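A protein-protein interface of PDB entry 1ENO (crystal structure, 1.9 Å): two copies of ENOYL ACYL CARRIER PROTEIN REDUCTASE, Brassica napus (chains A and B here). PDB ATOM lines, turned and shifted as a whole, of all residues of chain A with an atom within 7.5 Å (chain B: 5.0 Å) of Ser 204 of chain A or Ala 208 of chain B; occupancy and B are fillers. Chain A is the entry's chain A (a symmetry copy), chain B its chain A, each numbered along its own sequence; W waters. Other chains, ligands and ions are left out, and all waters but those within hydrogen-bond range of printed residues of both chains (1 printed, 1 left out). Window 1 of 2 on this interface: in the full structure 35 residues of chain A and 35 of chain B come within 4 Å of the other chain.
The backbone carbonyl oxygen (O) of Ser 191 of chain A lies within hydrogen-bond range of the side-chain hydroxyl (OG) of Ser 211 of chain B (2.8 Å).
OH of Tyr 155 of chain A sits at hydrogen-bond distance from OD2 of Asp 212 of chain B, 2.4 Å away.
OG of Ser 204 of chain A sits at hydrogen-bond distance from OD1 of Asp 212 of chain B (2.8 Å).
Water W1 lies within hydrogen-bond range of the side-chain hydroxyl (OG) of Ser 203 of chain A (2.5 Å), the side-chain carboxylate (OD1) of Asp 212 of chain B (2.7 Å) and the side-chain hydroxyl (OG) of Ser 211 of chain B (3.0 Å).
Hydrophobic or aromatic side chains of chain B that line the printed part of chain A: Ala 207 and Ala 208.
Along chain A the printed residues that touch a printed residue of chain B span positions 147 to 211.
Among the printed residues, 13 pairs touch across the chains.
Among the printed residues, no Asp or Glu carboxylate lies within 4 Å of a Lys or Arg side-chain nitrogen of the other chain.
OE2 of Glu 210 of chain A sits at hydrogen-bond distance from OG of Ser 191 of chain A (2.7 Å).
The side-chain hydroxyl of Ser 163 of chain B is in hydrogen-bond range of the backbone carbonyl oxygen of Ala 205 of chain B.
Printed residues of chain B within 4 Å of Ser 204 of chain A: Ala 208 (3.996 Å) and Asp 212 (2.8 Å).
Of the printed residues of chain B, Ala 207 of chain A touches Ala 207 and Ser 211.
Leu 209 of chain A touches none of the printed residues of chain B.
Printed residues of chain B within 4 Å of Ser 211 of chain A: Ala 207 (3.5 Å).
Of the printed residues of chain A, Ser 163 of chain B touches Tyr 155.
Of the printed residues of chain A, Ser 204 of chain B touches Ala 208.
Ala 207 of chain B touches just these residues of chain A: Ala 207 and Ser 211.
The nearest printed residue of chain B that does not touch Ser 204 of chain A is Ser 211 of chain B (4.4 Å).
The nearest printed residue of chain A that does not touch Ala 208 of chain B is Ala 207 of chain A (4.3 Å).
The nearest printed residue of chain B that does not touch Ser 203 of chain A is Asp 212 of chain B (4.5 Å).
Leu 147 of chain A touches Asp 212 of chain B (CD1 to OD1, 3.5 Å).
Tyr 155 of chain A touches Ser 163 of chain B.
Tyr 155 of chain A touches Ala 208 of chain B (OH to CB, 3.8 Å).
Ala 190 of chain A touches Ser 211 of chain B (O to OG, 3.8 Å).
Ser 203 of chain A touches Ser 211 of chain B (O to OG, 3.8 Å).
CB of Ala 208 of chain B touches O of Ser 204 of chain A, at 3.996 Å.
O of Ala 207 of chain A touches CB of Ala 207 of chain B, 3.6 Å away.
Ala 207 of chain A touches Ser 211 of chain B.
Ala 208 of chain A touches Ser 204 of chain B (CB to O, 3.996 Å).
Ser 211 of chain A touches Ala 207 of chain B.
Ser 204 of chain A touches Ala 208 of chain B, and with the chains exchanged Ala 208 of chain A touches Ser 204 of chain B.
Ala 207 of chain B touches its own counterpart, Ala 207 of chain A.
Ala 207 of chain A touches Ser 211 of chain B, and with the chains exchanged Ser 211 of chain A touches Ala 207 of chain B.
9 positions are printed for both chains.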
ATOM      1  N   LEU A 147     -16.811  17.136   8.428  1.00  0.00           N
ATOM      2  CA  LEU A 147     -15.652  16.310   8.249  1.00  0.00           C
ATOM      3  C   LEU A 147     -14.951  16.083   9.572  1.00  0.00           C
ATOM      4  O   LEU A 147     -14.451  15.013   9.834  1.00  0.00           O
ATOM      5  CB  LEU A 147     -14.622  16.919   7.256  1.00  0.00           C
ATOM      6  CG  LEU A 147     -14.842  16.569   5.825  1.00  0.00           C
ATOM      7  CD1 LEU A 147     -13.669  17.120   5.013  1.00  0.00           C
ATOM      8  CD2 LEU A 147     -14.960  15.075   5.626  1.00  0.00           C
ATOM      9  N   TYR A 155     -16.137   7.714   6.390  1.00  0.00           N
ATOM     10  CA  TYR A 155     -15.511   8.357   5.237  1.00  0.00           C
ATOM     11  C   TYR A 155     -15.240   7.350   4.069  1.00  0.00           C
ATOM     12  O   TYR A 155     -15.625   7.537   2.920  1.00  0.00           O
ATOM     13  CB  TYR A 155     -14.253   9.086   5.733  1.00  0.00           C
ATOM     14  CG  TYR A 155     -13.504   9.941   4.704  1.00  0.00           C
ATOM     15  CD1 TYR A 155     -12.637   9.357   3.769  1.00  0.00           C
ATOM     16  CD2 TYR A 155     -13.617  11.339   4.717  1.00  0.00           C
ATOM     17  CE1 TYR A 155     -11.804  10.143   2.944  1.00  0.00           C
ATOM     18  CE2 TYR A 155     -12.803  12.139   3.906  1.00  0.00           C
ATOM     19  CZ  TYR A 155     -11.886  11.542   3.028  1.00  0.00           C
ATOM     20  OH  TYR A 155     -11.083  12.318   2.218  1.00  0.00           O
ATOM     21  N   ALA A 158     -18.431   6.033   2.281  1.00  0.00           N
ATOM     22  CA  ALA A 158     -18.931   6.967   1.320  1.00  0.00           C
ATOM     23  C   ALA A 158     -18.120   6.888   0.011  1.00  0.00           C
ATOM     24  O   ALA A 158     -18.673   6.857  -1.073  1.00  0.00           O
ATOM     25  CB  ALA A 158     -18.917   8.362   1.905  1.00  0.00           C
ATOM     26  N   ILE A 159     -16.796   6.798   0.141  1.00  0.00           N
ATOM     27  CA  ILE A 159     -15.951   6.686  -1.016  1.00  0.00           C
ATOM     28  C   ILE A 159     -16.208   5.389  -1.735  1.00  0.00           C
ATOM     29  O   ILE A 159     -16.306   5.303  -2.948  1.00  0.00           O
ATOM     30  CB  ILE A 159     -14.484   6.715  -0.636  1.00  0.00           C
ATOM     31  CG1 ILE A 159     -14.118   7.976   0.115  1.00  0.00           C
ATOM     32  CG2 ILE A 159     -13.593   6.540  -1.872  1.00  0.00           C
ATOM     33  CD1 ILE A 159     -14.367   9.197  -0.716  1.00  0.00           C
ATOM     34  N   SER A 163     -17.785   6.520  -5.064  1.00  0.00           N
ATOM     35  CA  SER A 163     -16.694   6.719  -6.068  1.00  0.00           C
ATOM     36  C   SER A 163     -16.183   5.429  -6.678  1.00  0.00           C
ATOM     37  O   SER A 163     -16.246   5.223  -7.895  1.00  0.00           O
ATOM     38  CB  SER A 163     -15.464   7.525  -5.553  1.00  0.00           C
ATOM     39  OG  SER A 163     -15.863   8.607  -4.757  1.00  0.00           O
ATOM     40  N   ALA A 190     -20.188  20.325  -4.272  1.00  0.00           N
ATOM     41  CA  ALA A 190     -19.474  20.243  -3.014  1.00  0.00           C
ATOM     42  C   ALA A 190     -18.052  19.732  -3.219  1.00  0.00           C
ATOM     43  O   ALA A 190     -17.171  19.917  -2.370  1.00  0.00           O
ATOM     44  CB  ALA A 190     -20.212  19.365  -2.026  1.00  0.00           C
ATOM     45  N   SER A 191     -17.796  19.043  -4.340  1.00  0.00           N
ATOM     46  CA  SER A 191     -16.435  18.588  -4.607  1.00  0.00           C
ATOM     47  C   SER A 191     -15.416  19.753  -4.742  1.00  0.00           C
ATOM     48  O   SER A 191     -14.265  19.670  -4.298  1.00  0.00           O
ATOM     49  CB  SER A 191     -16.381  17.809  -5.887  1.00  0.00           C
ATOM     50  OG  SER A 191     -16.836  18.684  -6.878  1.00  0.00           O
ATOM     51  N   TYR A 198     -23.021  19.162   3.570  1.00  0.00           N
ATOM     52  CA  TYR A 198     -22.848  18.000   2.692  1.00  0.00           C
ATOM     53  C   TYR A 198     -21.669  17.232   3.283  1.00  0.00           C
ATOM     54  O   TYR A 198     -20.512  17.419   2.899  1.00  0.00           O
ATOM     55  CB  TYR A 198     -22.547  18.498   1.281  1.00  0.00           C
ATOM     56  CG  TYR A 198     -22.733  17.444   0.206  1.00  0.00           C
ATOM     57  CD1 TYR A 198     -23.998  17.023  -0.207  1.00  0.00           C
ATOM     58  CD2 TYR A 198     -21.612  16.876  -0.408  1.00  0.00           C
ATOM     59  CE1 TYR A 198     -24.129  16.046  -1.206  1.00  0.00           C
ATOM     60  CE2 TYR A 198     -21.717  15.936  -1.436  1.00  0.00           C
ATOM     61  CZ  TYR A 198     -22.989  15.530  -1.827  1.00  0.00           C
ATOM     62  OH  TYR A 198     -23.122  14.627  -2.830  1.00  0.00           O
ATOM     63  N   GLY A 199     -21.946  16.470   4.352  1.00  0.00           N
ATOM     64  CA  GLY A 199     -20.895  15.905   5.165  1.00  0.00           C
ATOM     65  C   GLY A 199     -20.542  14.496   4.905  1.00  0.00           C
ATOM     66  O   GLY A 199     -20.836  13.952   3.872  1.00  0.00           O
ATOM     67  N   GLY A 200     -19.857  13.940   5.891  1.00  0.00           N
ATOM     68  CA  GLY A 200     -19.510  12.562   5.925  1.00  0.00           C
ATOM     69  C   GLY A 200     -18.554  12.082   4.835  1.00  0.00           C
ATOM     70  O   GLY A 200     -18.496  10.897   4.567  1.00  0.00           O
ATOM     71  N   GLY A 201     -17.791  12.956   4.209  1.00  0.00           N
ATOM     72  CA  GLY A 201     -16.887  12.493   3.150  1.00  0.00           C
ATOM     73  C   GLY A 201     -17.602  12.376   1.817  1.00  0.00           C
ATOM     74  O   GLY A 201     -17.050  11.818   0.868  1.00  0.00           O
ATOM     75  N   MET A 202     -18.864  12.860   1.741  1.00  0.00           N
ATOM     76  CA  MET A 202     -19.578  12.818   0.476  1.00  0.00           C
ATOM     77  C   MET A 202     -18.970  13.872  -0.472  1.00  0.00           C
ATOM     78  O   MET A 202     -18.888  13.703  -1.693  1.00  0.00           O
ATOM     79  CB  MET A 202     -21.111  13.044   0.653  1.00  0.00           C
ATOM     80  CG  MET A 202     -21.860  11.811   1.084  1.00  0.00           C
ATOM     81  SD  MET A 202     -21.770  10.489  -0.168  1.00  0.00           S
ATOM     82  CE  MET A 202     -21.913  11.498  -1.632  1.00  0.00           C
ATOM     83  N   SER A 203     -18.503  14.999   0.111  1.00  0.00           N
ATOM     84  CA  SER A 203     -17.867  15.974  -0.762  1.00  0.00           C
ATOM     85  C   SER A 203     -16.561  15.341  -1.344  1.00  0.00           C
ATOM     86  O   SER A 203     -16.262  15.446  -2.545  1.00  0.00           O
ATOM     87  CB  SER A 203     -17.564  17.224   0.015  1.00  0.00           C
ATOM     88  OG  SER A 203     -16.763  16.865   1.128  1.00  0.00           O
ATOM     89  N   SER A 204     -15.816  14.635  -0.446  1.00  0.00           N
ATOM     90  CA  SER A 204     -14.595  13.937  -0.768  1.00  0.00           C
ATOM     91  C   SER A 204     -14.833  12.953  -1.888  1.00  0.00           C
ATOM     92  O   SER A 204     -14.041  12.849  -2.854  1.00  0.00           O
ATOM     93  CB  SER A 204     -14.080  13.229   0.468  1.00  0.00           C
ATOM     94  OG  SER A 204     -14.304  14.064   1.600  1.00  0.00           O
ATOM     95  N   ALA A 205     -15.949  12.222  -1.769  1.00  0.00           N
ATOM     96  CA  ALA A 205     -16.280  11.211  -2.734  1.00  0.00           C
ATOM     97  C   ALA A 205     -16.626  11.819  -4.053  1.00  0.00           C
ATOM     98  O   ALA A 205     -16.329  11.239  -5.065  1.00  0.00           O
ATOM     99  CB  ALA A 205     -17.425  10.363  -2.244  1.00  0.00           C
ATOM    100  N   LYS A 206     -17.302  12.952  -4.058  1.00  0.00           N
ATOM    101  CA  LYS A 206     -17.638  13.558  -5.363  1.00  0.00           C
ATOM    102  C   LYS A 206     -16.376  14.070  -6.050  1.00  0.00           C
ATOM    103  O   LYS A 206     -16.259  13.943  -7.246  1.00  0.00           O
ATOM    104  CB  LYS A 206     -18.629  14.695  -5.214  1.00  0.00           C
ATOM    105  CG  LYS A 206     -20.015  14.158  -4.805  1.00  0.00           C
ATOM    106  CD  LYS A 206     -20.555  13.115  -5.781  1.00  0.00           C
ATOM    107  CE  LYS A 206     -22.110  12.896  -5.571  1.00  0.00           C
ATOM    108  NZ  LYS A 206     -22.672  11.909  -6.522  1.00  0.00           N
ATOM    109  N   ALA A 207     -15.408  14.573  -5.246  1.00  0.00           N
ATOM    110  CA  ALA A 207     -14.108  15.017  -5.791  1.00  0.00           C
ATOM    111  C   ALA A 207     -13.384  13.838  -6.431  1.00  0.00           C
ATOM    112  O   ALA A 207     -12.883  13.922  -7.557  1.00  0.00           O
ATOM    113  CB  ALA A 207     -13.223  15.655  -4.716  1.00  0.00           C
ATOM    114  N   ALA A 208     -13.387  12.701  -5.768  1.00  0.00           N
ATOM    115  CA  ALA A 208     -12.714  11.521  -6.379  1.00  0.00           C
ATOM    116  C   ALA A 208     -13.426  11.093  -7.715  1.00  0.00           C
ATOM    117  O   ALA A 208     -12.817  10.777  -8.714  1.00  0.00           O
ATOM    118  CB  ALA A 208     -12.679  10.387  -5.359  1.00  0.00           C
ATOM    119  N   LEU A 209     -14.751  11.078  -7.691  1.00  0.00           N
ATOM    120  CA  LEU A 209     -15.525  10.659  -8.831  1.00  0.00           C
ATOM    121  C   LEU A 209     -15.195  11.542  -9.999  1.00  0.00           C
ATOM    122  O   LEU A 209     -15.068  11.068 -11.106  1.00  0.00           O
ATOM    123  CB  LEU A 209     -17.022  10.793  -8.517  1.00  0.00           C
ATOM    124  CG  LEU A 209     -17.984  10.384  -9.645  1.00  0.00           C
ATOM    125  CD1 LEU A 209     -18.030   8.875  -9.725  1.00  0.00           C
ATOM    126  CD2 LEU A 209     -19.387  10.869  -9.297  1.00  0.00           C
ATOM    127  N   GLU A 210     -15.122  12.879  -9.756  1.00  0.00           N
ATOM    128  CA  GLU A 210     -14.800  13.782 -10.865  1.00  0.00           C
ATOM    129  C   GLU A 210     -13.387  13.558 -11.441  1.00  0.00           C
ATOM    130  O   GLU A 210     -13.154  13.542 -12.655  1.00  0.00           O
ATOM    131  CB  GLU A 210     -15.035  15.257 -10.526  1.00  0.00           C
ATOM    132  CG  GLU A 210     -16.515  15.612 -10.211  1.00  0.00           C
ATOM    133  CD  GLU A 210     -16.646  17.018  -9.646  1.00  0.00           C
ATOM    134  OE1 GLU A 210     -15.768  17.870  -9.791  1.00  0.00           O
ATOM    135  OE2 GLU A 210     -17.674  17.214  -8.992  1.00  0.00           O
ATOM    136  N   SER A 211     -12.430  13.399 -10.562  1.00  0.00           N
ATOM    137  CA  SER A 211     -11.072  13.150 -10.974  1.00  0.00           C
ATOM    138  C   SER A 211     -10.964  11.844 -11.730  1.00  0.00           C
ATOM    139  O   SER A 211     -10.278  11.737 -12.734  1.00  0.00           O
ATOM    140  CB  SER A 211     -10.196  13.163  -9.707  1.00  0.00           C
ATOM    141  OG  SER A 211      -8.817  12.921  -9.975  1.00  0.00           O
ATOM    142  N   SER B 163      -5.482  10.504   2.129  1.00  0.00           N
ATOM    143  CA  SER B 163      -6.513  11.568   2.331  1.00  0.00           C
ATOM    144  C   SER B 163      -7.084  11.607   3.735  1.00  0.00           C
ATOM    145  O   SER B 163      -6.982  12.615   4.443  1.00  0.00           O
ATOM    146  CB  SER B 163      -7.707  11.527   1.331  1.00  0.00           C
ATOM    147  OG  SER B 163      -7.271  11.239   0.031  1.00  0.00           O
ATOM    148  N   SER B 204      -7.096   9.903  -7.256  1.00  0.00           N
ATOM    149  CA  SER B 204      -8.347   9.979  -6.541  1.00  0.00           C
ATOM    150  C   SER B 204      -8.128  10.558  -5.164  1.00  0.00           C
ATOM    151  O   SER B 204      -8.883  11.441  -4.691  1.00  0.00           O
ATOM    152  CB  SER B 204      -8.960   8.598  -6.451  1.00  0.00           C
ATOM    153  OG  SER B 204      -8.729   7.914  -7.678  1.00  0.00           O
ATOM    154  N   ALA B 205      -7.069  10.066  -4.506  1.00  0.00           N
ATOM    155  CA  ALA B 205      -6.766  10.488  -3.167  1.00  0.00           C
ATOM    156  C   ALA B 205      -6.324  11.914  -3.138  1.00  0.00           C
ATOM    157  O   ALA B 205      -6.617  12.602  -2.195  1.00  0.00           O
ATOM    158  CB  ALA B 205      -5.703   9.608  -2.561  1.00  0.00           C
ATOM    159  N   LYS B 206      -5.574  12.353  -4.131  1.00  0.00           N
ATOM    160  CA  LYS B 206      -5.143  13.766  -4.107  1.00  0.00           C
ATOM    161  C   LYS B 206      -6.338  14.688  -4.331  1.00  0.00           C
ATOM    162  O   LYS B 206      -6.412  15.722  -3.710  1.00  0.00           O
ATOM    163  CB  LYS B 206      -4.085  14.046  -5.156  1.00  0.00           C
ATOM    164  CG  LYS B 206      -2.757  13.356  -4.786  1.00  0.00           C
ATOM    165  CD  LYS B 206      -2.247  13.760  -3.404  1.00  0.00           C
ATOM    166  CE  LYS B 206      -0.721  13.373  -3.230  1.00  0.00           C
ATOM    167  NZ  LYS B 206      -0.186  13.776  -1.909  1.00  0.00           N
ATOM    168  N   ALA B 207      -7.303  14.240  -5.169  1.00  0.00           N
ATOM    169  CA  ALA B 207      -8.546  15.007  -5.393  1.00  0.00           C
ATOM    170  C   ALA B 207      -9.319  15.134  -4.085  1.00  0.00           C
ATOM    171  O   ALA B 207      -9.765  16.221  -3.702  1.00  0.00           O
ATOM    172  CB  ALA B 207      -9.431  14.366  -6.466  1.00  0.00           C
ATOM    173  N   ALA B 208      -9.421  14.054  -3.341  1.00  0.00           N
ATOM    174  CA  ALA B 208     -10.145  14.151  -2.043  1.00  0.00           C
ATOM    175  C   ALA B 208      -9.407  15.129  -1.056  1.00  0.00           C
ATOM    176  O   ALA B 208      -9.993  15.939  -0.370  1.00  0.00           O
ATOM    177  CB  ALA B 208     -10.299  12.751  -1.456  1.00  0.00           C
ATOM    178  N   LEU B 209      -8.088  15.012  -0.997  1.00  0.00           N
ATOM    179  CA  LEU B 209      -7.296  15.812  -0.098  1.00  0.00           C
ATOM    180  C   LEU B 209      -7.516  17.263  -0.411  1.00  0.00           C
ATOM    181  O   LEU B 209      -7.628  18.071   0.484  1.00  0.00           O
ATOM    182  CB  LEU B 209      -5.808  15.484  -0.289  1.00  0.00           C
ATOM    183  CG  LEU B 209      -4.829  16.266   0.602  1.00  0.00           C
ATOM    184  CD1 LEU B 209      -4.881  15.696   2.002  1.00  0.00           C
ATOM    185  CD2 LEU B 209      -3.413  16.062   0.075  1.00  0.00           C
ATOM    186  N   GLU B 210      -7.510  17.615  -1.725  1.00  0.00           N
ATOM    187  CA  GLU B 210      -7.723  19.021  -2.082  1.00  0.00           C
ATOM    188  C   GLU B 210      -9.122  19.541  -1.694  1.00  0.00           C
ATOM    189  O   GLU B 210      -9.303  20.647  -1.171  1.00  0.00           O
ATOM    190  CB  GLU B 210      -7.404  19.324  -3.549  1.00  0.00           C
ATOM    191  CG  GLU B 210      -5.918  19.090  -3.941  1.00  0.00           C
ATOM    192  CD  GLU B 210      -5.717  19.167  -5.447  1.00  0.00           C
ATOM    193  OE1 GLU B 210      -6.529  19.718  -6.192  1.00  0.00           O
ATOM    194  OE2 GLU B 210      -4.707  18.590  -5.859  1.00  0.00           O
ATOM    195  N   SER B 211     -10.124  18.744  -1.966  1.00  0.00           N
ATOM    196  CA  SER B 211     -11.477  19.102  -1.624  1.00  0.00           C
ATOM    197  C   SER B 211     -11.639  19.239  -0.125  1.00  0.00           C
ATOM    198  O   SER B 211     -12.288  20.146   0.371  1.00  0.00           O
ATOM    199  CB  SER B 211     -12.403  18.022  -2.213  1.00  0.00           C
ATOM    200  OG  SER B 211     -13.783  18.254  -1.939  1.00  0.00           O
ATOM    201  N   ASP B 212     -11.041  18.320   0.623  1.00  0.00           N
ATOM    202  CA  ASP B 212     -11.057  18.358   2.093  1.00  0.00           C
ATOM    203  C   ASP B 212     -10.341  19.573   2.631  1.00  0.00           C
ATOM    204  O   ASP B 212     -10.675  20.059   3.688  1.00  0.00           O
ATOM    205  CB  ASP B 212     -10.440  17.098   2.750  1.00  0.00           C
ATOM    206  CG  ASP B 212     -11.255  15.833   2.493  1.00  0.00           C
ATOM    207  OD1 ASP B 212     -12.377  16.041   1.927  1.00  0.00           O
ATOM    208  OD2 ASP B 212     -10.790  14.699   2.713  1.00  0.00           O
ATOM    209  N   THR B 213      -9.298  20.022   1.936  1.00  0.00           N
ATOM    210  CA  THR B 213      -8.600  21.226   2.361  1.00  0.00           C
ATOM    211  C   THR B 213      -9.549  22.407   2.445  1.00  0.00           C
ATOM    212  O   THR B 213      -9.497  23.189   3.342  1.00  0.00           O
ATOM    213  CB  THR B 213      -7.455  21.537   1.376  1.00  0.00           C
ATOM    214  OG1 THR B 213      -6.497  20.483   1.405  1.00  0.00           O
ATOM    215  CG2 THR B 213      -6.781  22.880   1.682  1.00  0.00           C
HETATM  216  O   HOH W   1     -14.378  17.522   0.955  1.00  0.00           O
